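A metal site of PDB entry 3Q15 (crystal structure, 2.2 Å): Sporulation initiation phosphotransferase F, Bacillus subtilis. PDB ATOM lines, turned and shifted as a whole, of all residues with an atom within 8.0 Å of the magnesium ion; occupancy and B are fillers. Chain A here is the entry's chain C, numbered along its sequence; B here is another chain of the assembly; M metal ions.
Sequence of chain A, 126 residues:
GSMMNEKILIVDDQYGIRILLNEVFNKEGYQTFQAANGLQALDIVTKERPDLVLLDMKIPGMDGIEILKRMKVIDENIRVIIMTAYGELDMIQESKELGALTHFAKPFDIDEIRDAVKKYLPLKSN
The side-chain amino group of Lys 106 lies within salt-bridge range of the side-chain carboxylate of Asp 56 (3.5 Å). The backbone NH of Asp 56 sits at hydrogen-bond distance from the backbone carbonyl oxygen of Val 11 (3.0 Å).
Within 4 Å of the magnesium ion: Asp 13, Asp 56 and Lys 58.
The magnesium ion is bound by the side-chain carboxylate of Asp 56 (2.1 Å), the side-chain carboxylate of Asp 13 (2.2 Å) and the backbone carbonyl oxygen of Lys 58 (2.3 Å). The magnesium ion has three donor atoms within binding distance.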
ATOM      1  N   VAL A  11     -21.066 -18.997  28.373  1.00  0.00           N
ATOM      2  CA  VAL A  11     -20.271 -17.966  29.046  1.00  0.00           C
ATOM      3  C   VAL A  11     -18.776 -18.240  28.936  1.00  0.00           C
ATOM      4  O   VAL A  11     -18.261 -19.222  29.491  1.00  0.00           O
ATOM      5  CB  VAL A  11     -20.656 -17.840  30.536  1.00  0.00           C
ATOM      6  CG1 VAL A  11     -19.906 -16.680  31.172  1.00  0.00           C
ATOM      7  CG2 VAL A  11     -22.163 -17.668  30.696  1.00  0.00           C
ATOM      8  N   ASP A  12     -18.071 -17.366  28.211  1.00  0.00           N
ATOM      9  CA  ASP A  12     -16.632 -17.500  28.038  1.00  0.00           C
ATOM     10  C   ASP A  12     -16.034 -16.200  27.508  1.00  0.00           C
ATOM     11  O   ASP A  12     -16.611 -15.548  26.619  1.00  0.00           O
ATOM     12  CB  ASP A  12     -16.294 -18.656  27.103  1.00  0.00           C
ATOM     13  CG  ASP A  12     -14.834 -19.077  27.191  1.00  0.00           C
ATOM     14  OD1 ASP A  12     -13.972 -18.376  26.627  1.00  0.00           O
ATOM     15  OD2 ASP A  12     -14.566 -20.114  27.841  1.00  0.00           O
ATOM     16  N   ASP A  13     -14.874 -15.825  28.035  1.00  0.00           N
ATOM     17  CA  ASP A  13     -14.247 -14.553  27.694  1.00  0.00           C
ATOM     18  C   ASP A  13     -13.510 -14.604  26.359  1.00  0.00           C
ATOM     19  O   ASP A  13     -13.068 -13.567  25.851  1.00  0.00           O
ATOM     20  CB  ASP A  13     -13.269 -14.137  28.801  1.00  0.00           C
ATOM     21  CG  ASP A  13     -12.083 -15.064  28.923  1.00  0.00           C
ATOM     22  OD1 ASP A  13     -12.265 -16.206  29.397  1.00  0.00           O
ATOM     23  OD2 ASP A  13     -10.970 -14.654  28.548  1.00  0.00           O
ATOM     24  N   GLN A  14     -13.377 -15.789  25.783  1.00  0.00           N
ATOM     25  CA  GLN A  14     -12.650 -15.935  24.534  1.00  0.00           C
ATOM     26  C   GLN A  14     -13.552 -16.199  23.329  1.00  0.00           C
ATOM     27  O   GLN A  14     -14.319 -17.153  23.301  1.00  0.00           O
ATOM     28  CB  GLN A  14     -11.560 -17.008  24.666  1.00  0.00           C
ATOM     29  CG  GLN A  14     -10.499 -16.660  25.718  1.00  0.00           C
ATOM     30  CD  GLN A  14      -9.260 -17.539  25.637  1.00  0.00           C
ATOM     31  OE1 GLN A  14      -9.202 -18.596  26.259  1.00  0.00           O
ATOM     32  NE2 GLN A  14      -8.266 -17.103  24.871  1.00  0.00           N
ATOM     33  N   ILE A  17     -13.957 -19.888  21.781  1.00  0.00           N
ATOM     34  CA  ILE A  17     -14.825 -20.852  22.452  1.00  0.00           C
ATOM     35  C   ILE A  17     -16.294 -20.564  22.180  1.00  0.00           C
ATOM     36  O   ILE A  17     -17.078 -21.480  21.913  1.00  0.00           O
ATOM     37  CB  ILE A  17     -14.584 -20.854  23.977  1.00  0.00           C
ATOM     38  CG1 ILE A  17     -13.117 -21.199  24.292  1.00  0.00           C
ATOM     39  CG2 ILE A  17     -15.528 -21.825  24.666  1.00  0.00           C
ATOM     40  CD1 ILE A  17     -12.705 -22.590  23.849  1.00  0.00           C
ATOM     41  N   ALA A  36     -19.535 -12.602  27.215  1.00  0.00           N
ATOM     42  CA  ALA A  36     -18.069 -12.559  27.313  1.00  0.00           C
ATOM     43  C   ALA A  36     -17.562 -12.409  28.743  1.00  0.00           C
ATOM     44  O   ALA A  36     -16.411 -12.747  29.030  1.00  0.00           O
ATOM     45  CB  ALA A  36     -17.510 -11.438  26.427  1.00  0.00           C
ATOM     46  N   LEU A  55     -20.321 -22.392  31.850  1.00  0.00           N
ATOM     47  CA  LEU A  55     -19.598 -21.300  32.491  1.00  0.00           C
ATOM     48  C   LEU A  55     -18.090 -21.519  32.537  1.00  0.00           C
ATOM     49  O   LEU A  55     -17.610 -22.510  33.095  1.00  0.00           O
ATOM     50  CB  LEU A  55     -20.142 -21.064  33.906  1.00  0.00           C
ATOM     51  CG  LEU A  55     -19.491 -19.951  34.745  1.00  0.00           C
ATOM     52  CD1 LEU A  55     -19.658 -18.593  34.095  1.00  0.00           C
ATOM     53  CD2 LEU A  55     -20.070 -19.939  36.159  1.00  0.00           C
ATOM     54  N   ASP A  56     -17.348 -20.593  31.944  1.00  0.00           N
ATOM     55  CA  ASP A  56     -15.889 -20.601  32.026  1.00  0.00           C
ATOM     56  C   ASP A  56     -15.444 -20.020  33.367  1.00  0.00           C
ATOM     57  O   ASP A  56     -15.613 -18.831  33.620  1.00  0.00           O
ATOM     58  CB  ASP A  56     -15.280 -19.787  30.888  1.00  0.00           C
ATOM     59  CG  ASP A  56     -13.766 -19.626  31.037  1.00  0.00           C
ATOM     60  OD1 ASP A  56     -13.268 -18.489  30.875  1.00  0.00           O
ATOM     61  OD2 ASP A  56     -13.085 -20.639  31.302  1.00  0.00           O
ATOM     62  N   MET A  57     -14.879 -20.855  34.219  1.00  0.00           N
ATOM     63  CA  MET A  57     -14.449 -20.419  35.542  1.00  0.00           C
ATOM     64  C   MET A  57     -13.182 -19.550  35.463  1.00  0.00           C
ATOM     65  O   MET A  57     -12.750 -18.968  36.457  1.00  0.00           O
ATOM     66  CB  MET A  57     -14.216 -21.611  36.456  1.00  0.00           C
ATOM     67  CG  MET A  57     -15.405 -22.567  36.541  1.00  0.00           C
ATOM     68  SD  MET A  57     -16.878 -21.773  37.203  1.00  0.00           S
ATOM     69  CE  MET A  57     -16.383 -21.496  38.906  1.00  0.00           C
ATOM     70  N   LYS A  58     -12.602 -19.476  34.263  1.00  0.00           N
ATOM     71  CA  LYS A  58     -11.382 -18.704  34.060  1.00  0.00           C
ATOM     72  C   LYS A  58     -11.665 -17.417  33.280  1.00  0.00           C
ATOM     73  O   LYS A  58     -11.348 -17.308  32.096  1.00  0.00           O
ATOM     74  CB  LYS A  58     -10.325 -19.539  33.333  1.00  0.00           C
ATOM     75  CG  LYS A  58      -9.031 -18.802  33.044  1.00  0.00           C
ATOM     76  CD  LYS A  58      -8.398 -18.265  34.318  1.00  0.00           C
ATOM     77  CE  LYS A  58      -7.145 -17.464  34.024  1.00  0.00           C
ATOM     78  NZ  LYS A  58      -6.127 -18.262  33.275  1.00  0.00           N
ATOM     79  N   ILE A  59     -12.274 -16.450  33.960  1.00  0.00           N
ATOM     80  CA  ILE A  59     -12.579 -15.158  33.352  1.00  0.00           C
ATOM     81  C   ILE A  59     -11.919 -14.038  34.151  1.00  0.00           C
ATOM     82  O   ILE A  59     -12.055 -13.968  35.374  1.00  0.00           O
ATOM     83  CB  ILE A  59     -14.099 -14.927  33.281  1.00  0.00           C
ATOM     84  CG1 ILE A  59     -14.765 -16.037  32.470  1.00  0.00           C
ATOM     85  CG2 ILE A  59     -14.409 -13.563  32.665  1.00  0.00           C
ATOM     86  CD1 ILE A  59     -16.271 -15.863  32.301  1.00  0.00           C
ATOM     87  N   PRO A  60     -11.195 -13.153  33.449  1.00  0.00           N
ATOM     88  CA  PRO A  60     -10.437 -12.050  34.064  1.00  0.00           C
ATOM     89  C   PRO A  60     -11.311 -11.069  34.834  1.00  0.00           C
ATOM     90  O   PRO A  60     -12.363 -10.663  34.338  1.00  0.00           O
ATOM     91  CB  PRO A  60      -9.812 -11.348  32.862  1.00  0.00           C
ATOM     92  CG  PRO A  60      -9.773 -12.375  31.788  1.00  0.00           C
ATOM     93  CD  PRO A  60     -10.996 -13.199  31.989  1.00  0.00           C
ATOM     94  N   MET A  83     -16.461 -25.296  32.786  1.00  0.00           N
ATOM     95  CA  MET A  83     -15.360 -25.724  31.949  1.00  0.00           C
ATOM     96  C   MET A  83     -14.126 -24.908  32.297  1.00  0.00           C
ATOM     97  O   MET A  83     -14.223 -23.718  32.585  1.00  0.00           O
ATOM     98  CB  MET A  83     -15.719 -25.558  30.473  1.00  0.00           C
ATOM     99  CG  MET A  83     -16.273 -24.188  30.126  1.00  0.00           C
ATOM    100  SD  MET A  83     -16.984 -24.116  28.479  1.00  0.00           S
ATOM    101  CE  MET A  83     -17.468 -22.388  28.420  1.00  0.00           C
ATOM    102  N   THR A  84     -12.960 -25.555  32.292  1.00  0.00           N
ATOM    103  CA  THR A  84     -11.747 -24.887  32.721  1.00  0.00           C
ATOM    104  C   THR A  84     -10.540 -25.227  31.853  1.00  0.00           C
ATOM    105  O   THR A  84     -10.486 -26.277  31.213  1.00  0.00           O
ATOM    106  CB  THR A  84     -11.401 -25.229  34.184  1.00  0.00           C
ATOM    107  OG1 THR A  84     -10.529 -24.226  34.717  1.00  0.00           O
ATOM    108  CG2 THR A  84     -10.727 -26.581  34.274  1.00  0.00           C
ATOM    109  N   ALA A  85      -9.571 -24.316  31.832  1.00  0.00           N
ATOM    110  CA  ALA A  85      -8.311 -24.536  31.155  1.00  0.00           C
ATOM    111  C   ALA A  85      -7.180 -24.342  32.160  1.00  0.00           C
ATOM    112  O   ALA A  85      -6.918 -23.220  32.606  1.00  0.00           O
ATOM    113  CB  ALA A  85      -8.152 -23.578  29.991  1.00  0.00           C
ATOM    114  N   LYS A 106     -10.547 -28.259  29.311  1.00  0.00           N
ATOM    115  CA  LYS A 106     -10.148 -27.834  27.968  1.00  0.00           C
ATOM    116  C   LYS A 106      -8.794 -28.458  27.617  1.00  0.00           C
ATOM    117  O   LYS A 106      -7.908 -28.544  28.471  1.00  0.00           O
ATOM    118  CB  LYS A 106     -10.063 -26.313  27.899  1.00  0.00           C
ATOM    119  CG  LYS A 106     -11.380 -25.596  28.154  1.00  0.00           C
ATOM    120  CD  LYS A 106     -11.212 -24.093  28.041  1.00  0.00           C
ATOM    121  CE  LYS A 106     -12.530 -23.368  28.229  1.00  0.00           C
ATOM    122  NZ  LYS A 106     -12.356 -21.893  28.113  1.00  0.00           N
ATOM    123  N   GLN B  49      -3.636 -21.386  26.507  1.00  0.00           N
ATOM    124  CA  GLN B  49      -5.055 -21.617  26.263  1.00  0.00           C
ATOM    125  C   GLN B  49      -5.480 -21.185  24.861  1.00  0.00           C
ATOM    126  O   GLN B  49      -6.497 -21.656  24.348  1.00  0.00           O
ATOM    127  CB  GLN B  49      -5.913 -20.949  27.331  1.00  0.00           C
ATOM    128  CG  GLN B  49      -5.730 -19.452  27.452  1.00  0.00           C
ATOM    129  CD  GLN B  49      -6.560 -18.836  28.568  1.00  0.00           C
ATOM    130  OE1 GLN B  49      -6.315 -17.717  29.005  1.00  0.00           O
ATOM    131  NE2 GLN B  49      -7.563 -19.576  29.043  1.00  0.00           N
ATOM    132  N   ILE B  53      -7.593 -23.493  22.078  1.00  0.00           N
ATOM    133  CA  ILE B  53      -8.765 -23.021  21.358  1.00  0.00           C
ATOM    134  C   ILE B  53      -8.611 -23.311  19.876  1.00  0.00           C
ATOM    135  O   ILE B  53      -9.531 -23.816  19.231  1.00  0.00           O
ATOM    136  CB  ILE B  53      -8.982 -21.515  21.547  1.00  0.00           C
ATOM    137  CG1 ILE B  53      -9.311 -21.197  23.007  1.00  0.00           C
ATOM    138  CG2 ILE B  53     -10.088 -21.013  20.627  1.00  0.00           C
ATOM    139  CD1 ILE B  53      -9.606 -19.736  23.251  1.00  0.00           C
ATOM    140  N   TYR B 177     -10.175  -6.147  33.254  1.00  0.00           N
ATOM    141  CA  TYR B 177      -8.895  -6.621  32.743  1.00  0.00           C
ATOM    142  C   TYR B 177      -7.716  -5.872  33.367  1.00  0.00           C
ATOM    143  O   TYR B 177      -6.853  -5.358  32.656  1.00  0.00           O
ATOM    144  CB  TYR B 177      -8.845  -6.505  31.215  1.00  0.00           C
ATOM    145  CG  TYR B 177      -9.591  -7.611  30.491  1.00  0.00           C
ATOM    146  CD1 TYR B 177     -10.965  -7.540  30.294  1.00  0.00           C
ATOM    147  CD2 TYR B 177      -8.922  -8.724  30.000  1.00  0.00           C
ATOM    148  CE1 TYR B 177     -11.646  -8.548  29.636  1.00  0.00           C
ATOM    149  CE2 TYR B 177      -9.603  -9.733  29.342  1.00  0.00           C
ATOM    150  CZ  TYR B 177     -10.955  -9.638  29.161  1.00  0.00           C
ATOM    151  OH  TYR B 177     -11.638 -10.637  28.504  1.00  0.00           O
HETATM  152 MG    MG M   1     -11.431 -18.112  29.970  1.00  0.00          MG
